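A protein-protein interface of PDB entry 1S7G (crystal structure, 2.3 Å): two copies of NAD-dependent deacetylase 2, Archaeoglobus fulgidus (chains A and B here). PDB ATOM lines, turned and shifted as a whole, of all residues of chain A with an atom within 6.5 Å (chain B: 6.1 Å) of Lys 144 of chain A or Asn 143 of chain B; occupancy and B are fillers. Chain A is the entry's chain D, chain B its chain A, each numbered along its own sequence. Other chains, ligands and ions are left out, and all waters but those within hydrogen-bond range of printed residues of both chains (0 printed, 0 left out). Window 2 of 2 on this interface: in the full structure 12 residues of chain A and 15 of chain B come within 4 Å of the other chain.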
ATOM      1  N   MET A  68     -17.884   4.008   3.245  1.00  0.00           N
ATOM      2  CA  MET A  68     -19.183   4.680   3.252  1.00  0.00           C
ATOM      3  C   MET A  68     -19.267   5.775   2.195  1.00  0.00           C
ATOM      4  O   MET A  68     -20.272   5.897   1.501  1.00  0.00           O
ATOM      5  CB  MET A  68     -19.468   5.303   4.623  1.00  0.00           C
ATOM      6  CG  MET A  68     -19.782   4.306   5.720  1.00  0.00           C
ATOM      7  SD  MET A  68     -20.096   5.125   7.284  1.00  0.00           S
ATOM      8  CE  MET A  68     -20.114   3.727   8.392  1.00  0.00           C
ATOM      9  N   LYS A  71     -19.568   4.196  -1.300  1.00  0.00           N
ATOM     10  CA  LYS A  71     -20.552   3.121  -1.452  1.00  0.00           C
ATOM     11  C   LYS A  71     -21.206   2.990  -2.823  1.00  0.00           C
ATOM     12  O   LYS A  71     -21.660   1.905  -3.185  1.00  0.00           O
ATOM     13  CB  LYS A  71     -21.631   3.204  -0.362  1.00  0.00           C
ATOM     14  CG  LYS A  71     -22.480   4.463  -0.341  1.00  0.00           C
ATOM     15  CD  LYS A  71     -23.449   4.402   0.843  1.00  0.00           C
ATOM     16  CE  LYS A  71     -24.338   5.639   0.932  1.00  0.00           C
ATOM     17  NZ  LYS A  71     -25.370   5.526   2.015  1.00  0.00           N
ATOM     18  N   VAL A 139     -25.050  -4.356   7.019  1.00  0.00           N
ATOM     19  CA  VAL A 139     -25.541  -3.542   5.907  1.00  0.00           C
ATOM     20  C   VAL A 139     -26.481  -2.419   6.339  1.00  0.00           C
ATOM     21  O   VAL A 139     -26.460  -1.331   5.765  1.00  0.00           O
ATOM     22  CB  VAL A 139     -26.247  -4.426   4.840  1.00  0.00           C
ATOM     23  CG1 VAL A 139     -27.566  -4.954   5.383  1.00  0.00           C
ATOM     24  CG2 VAL A 139     -26.456  -3.638   3.564  1.00  0.00           C
ATOM     25  N   GLU A 140     -27.293  -2.682   7.356  1.00  0.00           N
ATOM     26  CA  GLU A 140     -28.235  -1.690   7.862  1.00  0.00           C
ATOM     27  C   GLU A 140     -27.484  -0.532   8.527  1.00  0.00           C
ATOM     28  O   GLU A 140     -27.672   0.629   8.163  1.00  0.00           O
ATOM     29  CB  GLU A 140     -29.188  -2.347   8.867  1.00  0.00           C
ATOM     30  CG  GLU A 140     -30.420  -1.531   9.208  1.00  0.00           C
ATOM     31  CD  GLU A 140     -31.340  -1.322   8.012  1.00  0.00           C
ATOM     32  OE1 GLU A 140     -31.604  -2.301   7.273  1.00  0.00           O
ATOM     33  OE2 GLU A 140     -31.808  -0.179   7.818  1.00  0.00           O
ATOM     34  N   ASP A 141     -26.637  -0.852   9.500  1.00  0.00           N
ATOM     35  CA  ASP A 141     -25.851   0.158  10.208  1.00  0.00           C
ATOM     36  C   ASP A 141     -24.960   0.928   9.235  1.00  0.00           C
ATOM     37  O   ASP A 141     -24.852   2.148   9.302  1.00  0.00           O
ATOM     38  CB  ASP A 141     -24.974  -0.509  11.270  1.00  0.00           C
ATOM     39  CG  ASP A 141     -25.761  -0.954  12.490  1.00  0.00           C
ATOM     40  OD1 ASP A 141     -25.217  -1.758  13.283  1.00  0.00           O
ATOM     41  OD2 ASP A 141     -26.913  -0.493  12.663  1.00  0.00           O
ATOM     42  N   PHE A 142     -24.319   0.192   8.335  1.00  0.00           N
ATOM     43  CA  PHE A 142     -23.430   0.778   7.341  1.00  0.00           C
ATOM     44  C   PHE A 142     -24.124   1.906   6.583  1.00  0.00           C
ATOM     45  O   PHE A 142     -23.665   3.045   6.591  1.00  0.00           O
ATOM     46  CB  PHE A 142     -22.982  -0.299   6.346  1.00  0.00           C
ATOM     47  CG  PHE A 142     -21.995   0.188   5.323  1.00  0.00           C
ATOM     48  CD1 PHE A 142     -20.674   0.453   5.681  1.00  0.00           C
ATOM     49  CD2 PHE A 142     -22.381   0.371   4.000  1.00  0.00           C
ATOM     50  CE1 PHE A 142     -19.754   0.890   4.734  1.00  0.00           C
ATOM     51  CE2 PHE A 142     -21.472   0.808   3.046  1.00  0.00           C
ATOM     52  CZ  PHE A 142     -20.155   1.067   3.411  1.00  0.00           C
ATOM     53  N   ASN A 143     -25.236   1.574   5.931  1.00  0.00           N
ATOM     54  CA  ASN A 143     -25.991   2.551   5.156  1.00  0.00           C
ATOM     55  C   ASN A 143     -26.606   3.674   5.988  1.00  0.00           C
ATOM     56  O   ASN A 143     -26.995   4.704   5.449  1.00  0.00           O
ATOM     57  CB  ASN A 143     -27.050   1.834   4.317  1.00  0.00           C
ATOM     58  CG  ASN A 143     -26.439   1.103   3.139  1.00  0.00           C
ATOM     59  OD1 ASN A 143     -25.822   1.722   2.267  1.00  0.00           O
ATOM     60  ND2 ASN A 143     -26.590  -0.218   3.110  1.00  0.00           N
ATOM     61  N   LYS A 144     -26.680   3.487   7.300  1.00  0.00           N
ATOM     62  CA  LYS A 144     -27.209   4.532   8.173  1.00  0.00           C
ATOM     63  C   LYS A 144     -26.028   5.425   8.568  1.00  0.00           C
ATOM     64  O   LYS A 144     -26.186   6.420   9.278  1.00  0.00           O
ATOM     65  CB  LYS A 144     -27.860   3.913   9.416  1.00  0.00           C
ATOM     66  CG  LYS A 144     -28.392   4.919  10.443  1.00  0.00           C
ATOM     67  CD  LYS A 144     -29.056   4.200  11.625  1.00  0.00           C
ATOM     68  CE  LYS A 144     -29.315   5.130  12.813  1.00  0.00           C
ATOM     69  NZ  LYS A 144     -30.383   6.148  12.585  1.00  0.00           N
ATOM     70  N   GLY A 145     -24.837   5.052   8.095  1.00  0.00           N
ATOM     71  CA  GLY A 145     -23.634   5.817   8.382  1.00  0.00           C
ATOM     72  C   GLY A 145     -22.931   5.461   9.681  1.00  0.00           C
ATOM     73  O   GLY A 145     -22.075   6.218  10.150  1.00  0.00           O
ATOM     74  N   GLU A 146     -23.286   4.319  10.267  1.00  0.00           N
ATOM     75  CA  GLU A 146     -22.678   3.877  11.523  1.00  0.00           C
ATOM     76  C   GLU A 146     -21.663   2.766  11.290  1.00  0.00           C
ATOM     77  O   GLU A 146     -21.929   1.796  10.570  1.00  0.00           O
ATOM     78  CB  GLU A 146     -23.752   3.385  12.495  1.00  0.00           C
ATOM     79  CG  GLU A 146     -24.775   4.443  12.889  1.00  0.00           C
ATOM     80  CD  GLU A 146     -25.777   3.920  13.903  1.00  0.00           C
ATOM     81  OE1 GLU A 146     -25.370   3.576  15.036  1.00  0.00           O
ATOM     82  OE2 GLU A 146     -26.974   3.844  13.569  1.00  0.00           O
ATOM     83  N   LEU B  74     -34.493  -1.107   6.242  1.00  0.00           N
ATOM     84  CA  LEU B  74     -34.676  -0.272   5.058  1.00  0.00           C
ATOM     85  C   LEU B  74     -33.715  -0.702   3.955  1.00  0.00           C
ATOM     86  O   LEU B  74     -33.969  -0.465   2.771  1.00  0.00           O
ATOM     87  CB  LEU B  74     -34.435   1.201   5.398  1.00  0.00           C
ATOM     88  CG  LEU B  74     -35.450   1.846   6.345  1.00  0.00           C
ATOM     89  CD1 LEU B  74     -34.960   3.225   6.784  1.00  0.00           C
ATOM     90  CD2 LEU B  74     -36.800   1.942   5.647  1.00  0.00           C
ATOM     91  N   PHE B  75     -32.611  -1.333   4.336  1.00  0.00           N
ATOM     92  CA  PHE B  75     -31.646  -1.771   3.340  1.00  0.00           C
ATOM     93  C   PHE B  75     -31.542  -3.281   3.249  1.00  0.00           C
ATOM     94  O   PHE B  75     -30.505  -3.825   2.868  1.00  0.00           O
ATOM     95  CB  PHE B  75     -30.277  -1.150   3.615  1.00  0.00           C
ATOM     96  CG  PHE B  75     -30.289   0.345   3.570  1.00  0.00           C
ATOM     97  CD1 PHE B  75     -30.615   1.086   4.701  1.00  0.00           C
ATOM     98  CD2 PHE B  75     -30.023   1.018   2.381  1.00  0.00           C
ATOM     99  CE1 PHE B  75     -30.677   2.477   4.647  1.00  0.00           C
ATOM    100  CE2 PHE B  75     -30.084   2.409   2.317  1.00  0.00           C
ATOM    101  CZ  PHE B  75     -30.411   3.139   3.453  1.00  0.00           C
ATOM    102  N   PHE B 138     -34.844   9.465  -0.771  1.00  0.00           N
ATOM    103  CA  PHE B 138     -35.318   9.830   0.566  1.00  0.00           C
ATOM    104  C   PHE B 138     -34.927   8.858   1.680  1.00  0.00           C
ATOM    105  O   PHE B 138     -34.982   9.215   2.852  1.00  0.00           O
ATOM    106  CB  PHE B 138     -36.852   9.934   0.584  1.00  0.00           C
ATOM    107  CG  PHE B 138     -37.415  10.994  -0.314  1.00  0.00           C
ATOM    108  CD1 PHE B 138     -37.275  12.337   0.000  1.00  0.00           C
ATOM    109  CD2 PHE B 138     -38.113  10.643  -1.465  1.00  0.00           C
ATOM    110  CE1 PHE B 138     -37.821  13.318  -0.816  1.00  0.00           C
ATOM    111  CE2 PHE B 138     -38.664  11.617  -2.289  1.00  0.00           C
ATOM    112  CZ  PHE B 138     -38.519  12.959  -1.964  1.00  0.00           C
ATOM    113  N   VAL B 139     -34.563   7.631   1.327  1.00  0.00           N
ATOM    114  CA  VAL B 139     -34.230   6.622   2.332  1.00  0.00           C
ATOM    115  C   VAL B 139     -33.390   7.097   3.508  1.00  0.00           C
ATOM    116  O   VAL B 139     -33.807   6.987   4.663  1.00  0.00           O
ATOM    117  CB  VAL B 139     -33.514   5.404   1.712  1.00  0.00           C
ATOM    118  CG1 VAL B 139     -34.454   4.226   1.681  1.00  0.00           C
ATOM    119  CG2 VAL B 139     -33.017   5.736   0.321  1.00  0.00           C
ATOM    120  N   GLU B 140     -32.210   7.622   3.214  1.00  0.00           N
ATOM    121  CA  GLU B 140     -31.314   8.088   4.258  1.00  0.00           C
ATOM    122  C   GLU B 140     -31.856   9.255   5.083  1.00  0.00           C
ATOM    123  O   GLU B 140     -31.710   9.265   6.304  1.00  0.00           O
ATOM    124  CB  GLU B 140     -29.954   8.420   3.641  1.00  0.00           C
ATOM    125  CG  GLU B 140     -29.325   7.195   2.986  1.00  0.00           C
ATOM    126  CD  GLU B 140     -27.948   7.455   2.417  1.00  0.00           C
ATOM    127  OE1 GLU B 140     -27.064   7.914   3.176  1.00  0.00           O
ATOM    128  OE2 GLU B 140     -27.748   7.187   1.211  1.00  0.00           O
ATOM    129  N   ASP B 141     -32.490  10.228   4.435  1.00  0.00           N
ATOM    130  CA  ASP B 141     -33.047  11.366   5.173  1.00  0.00           C
ATOM    131  C   ASP B 141     -34.124  10.834   6.120  1.00  0.00           C
ATOM    132  O   ASP B 141     -34.241  11.258   7.274  1.00  0.00           O
ATOM    133  CB  ASP B 141     -33.691  12.389   4.225  1.00  0.00           C
ATOM    134  CG  ASP B 141     -32.795  12.768   3.056  1.00  0.00           C
ATOM    135  OD1 ASP B 141     -33.084  13.798   2.404  1.00  0.00           O
ATOM    136  OD2 ASP B 141     -31.818  12.040   2.773  1.00  0.00           O
ATOM    137  N   PHE B 142     -34.913   9.898   5.604  1.00  0.00           N
ATOM    138  CA  PHE B 142     -35.993   9.274   6.355  1.00  0.00           C
ATOM    139  C   PHE B 142     -35.439   8.481   7.534  1.00  0.00           C
ATOM    140  O   PHE B 142     -36.017   8.492   8.621  1.00  0.00           O
ATOM    141  CB  PHE B 142     -36.800   8.375   5.409  1.00  0.00           C
ATOM    142  CG  PHE B 142     -37.788   7.476   6.096  1.00  0.00           C
ATOM    143  CD1 PHE B 142     -37.464   6.153   6.375  1.00  0.00           C
ATOM    144  CD2 PHE B 142     -39.057   7.934   6.421  1.00  0.00           C
ATOM    145  CE1 PHE B 142     -38.392   5.300   6.963  1.00  0.00           C
ATOM    146  CE2 PHE B 142     -39.990   7.086   7.010  1.00  0.00           C
ATOM    147  CZ  PHE B 142     -39.658   5.769   7.280  1.00  0.00           C
ATOM    148  N   ASN B 143     -34.309   7.813   7.320  1.00  0.00           N
ATOM    149  CA  ASN B 143     -33.684   7.016   8.373  1.00  0.00           C
ATOM    150  C   ASN B 143     -33.154   7.905   9.497  1.00  0.00           C
ATOM    151  O   ASN B 143     -32.901   7.434  10.602  1.00  0.00           O
ATOM    152  CB  ASN B 143     -32.547   6.166   7.795  1.00  0.00           C
ATOM    153  CG  ASN B 143     -32.181   4.992   8.689  1.00  0.00           C
ATOM    154  OD1 ASN B 143     -31.344   4.160   8.330  1.00  0.00           O
ATOM    155  ND2 ASN B 143     -32.810   4.916   9.859  1.00  0.00           N
ATOM    156  N   LYS B 144     -32.992   9.192   9.209  1.00  0.00           N
ATOM    157  CA  LYS B 144     -32.517  10.144  10.204  1.00  0.00           C
ATOM    158  C   LYS B 144     -33.717  10.843  10.845  1.00  0.00           C
ATOM    159  O   LYS B 144     -33.558  11.769  11.643  1.00  0.00           O
ATOM    160  CB  LYS B 144     -31.599  11.168   9.552  1.00  0.00           C
ATOM    161  N   GLY B 145     -34.918  10.397  10.481  1.00  0.00           N
ATOM    162  CA  GLY B 145     -36.135  10.979  11.023  1.00  0.00           C
ATOM    163  C   GLY B 145     -36.646  12.166  10.228  1.00  0.00           C
ATOM    164  O   GLY B 145     -37.487  12.929  10.705  1.00  0.00           O
ATOM    165  N   GLU B 146     -36.148  12.320   9.008  1.00  0.00           N
ATOM    166  CA  GLU B 146     -36.555  13.438   8.166  1.00  0.00           C
ATOM    167  C   GLU B 146     -37.694  13.066   7.216  1.00  0.00           C
ATOM    168  O   GLU B 146     -37.526  12.238   6.319  1.00  0.00           O
ATOM    169  CB  GLU B 146     -35.351  13.948   7.364  1.00  0.00           C
ATOM    170  CG  GLU B 146     -35.484  15.386   6.879  1.00  0.00           C
ATOM    171  CD  GLU B 146     -34.275  15.848   6.076  1.00  0.00           C
ATOM    172  OE1 GLU B 146     -33.138  15.747   6.594  1.00  0.00           O
ATOM    173  OE2 GLU B 146     -34.465  16.315   4.931  1.00  0.00           O
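The backbone NH (N) of Leu 74 of chain B sits at hydrogen-bond distance from the side-chain carboxylate (OE2) of Glu 140 of chain A, 3.2 Å away.
OE1 of Glu 140 of chain A lies within hydrogen-bond range of N of Phe 75 of chain B, 3.3 Å away.
The side-chain carboxylate (OE2) of Glu 140 of chain B lies within salt-bridge range of the side-chain amino group (NZ) of Lys 71 of chain A (3.0 Å).
O of Asn 143 of chain B sits at hydrogen-bond distance from NZ of Lys 144 of chain A (3.5 Å).
The side-chain amide nitrogen (ND2) of Asn 143 of chain A lies within hydrogen-bond range of the backbone carbonyl oxygen (O) of Val 139 of chain A, at 2.9 Å.
Asn 143 of chain A touches Phe 75 of chain B.
OE1 of Glu 140 of chain B touches O of Asn 143 of chain A (3.9 Å).
Of the printed residues of chain B, Lys 144 of chain A touches Asn 143 (3.5 Å).
Of chain A, only Lys 144 (3.5 Å) comes within 4 Å of Asn 143 of chain B.
Of the printed residues of chain A, Glu 140 of chain B touches Lys 71 (3.0 Å) and Asn 143 (3.9 Å).
Of the printed residues of chain A, Phe 75 of chain B touches Glu 140 (3.3 Å) and Asn 143 (3.6 Å).
Printed residues of chain A within 4 Å of Leu 74 of chain B: Glu 140 (3.2 Å).
Printed residues of chain B within 4 Å of Lys 71 of chain A: Glu 140.
Printed residues of chain B within 4 Å of Asn 143 of chain A: Phe 75 and Glu 140.
Phe 138 of chain B touches none of the printed residues of chain A.
The nearest residue of chain A that does not touch Asn 143 of chain B is Glu 140 of chain A (4.4 Å).
The nearest printed residue of chain B that does not touch Lys 71 of chain A is Phe 75 of chain B (5.7 Å).
Hydrophobic or aromatic side chains of chain B within 4 Å of the printed part of chain A: Leu 74 and Phe 75.
Along chain B the printed residues that touch a printed residue of chain A span positions 74 to 143.
Asn 143 of chain A touches Glu 140 of chain B, but with the chains exchanged Glu 140 of chain A does not touch Asn 143 of chain B (4.4 Å).
Lys 144 of chain A touches Asn 143 of chain B, but with the chains exchanged Asn 143 of chain A does not touch Lys 144 of chain B (8.4 Å).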
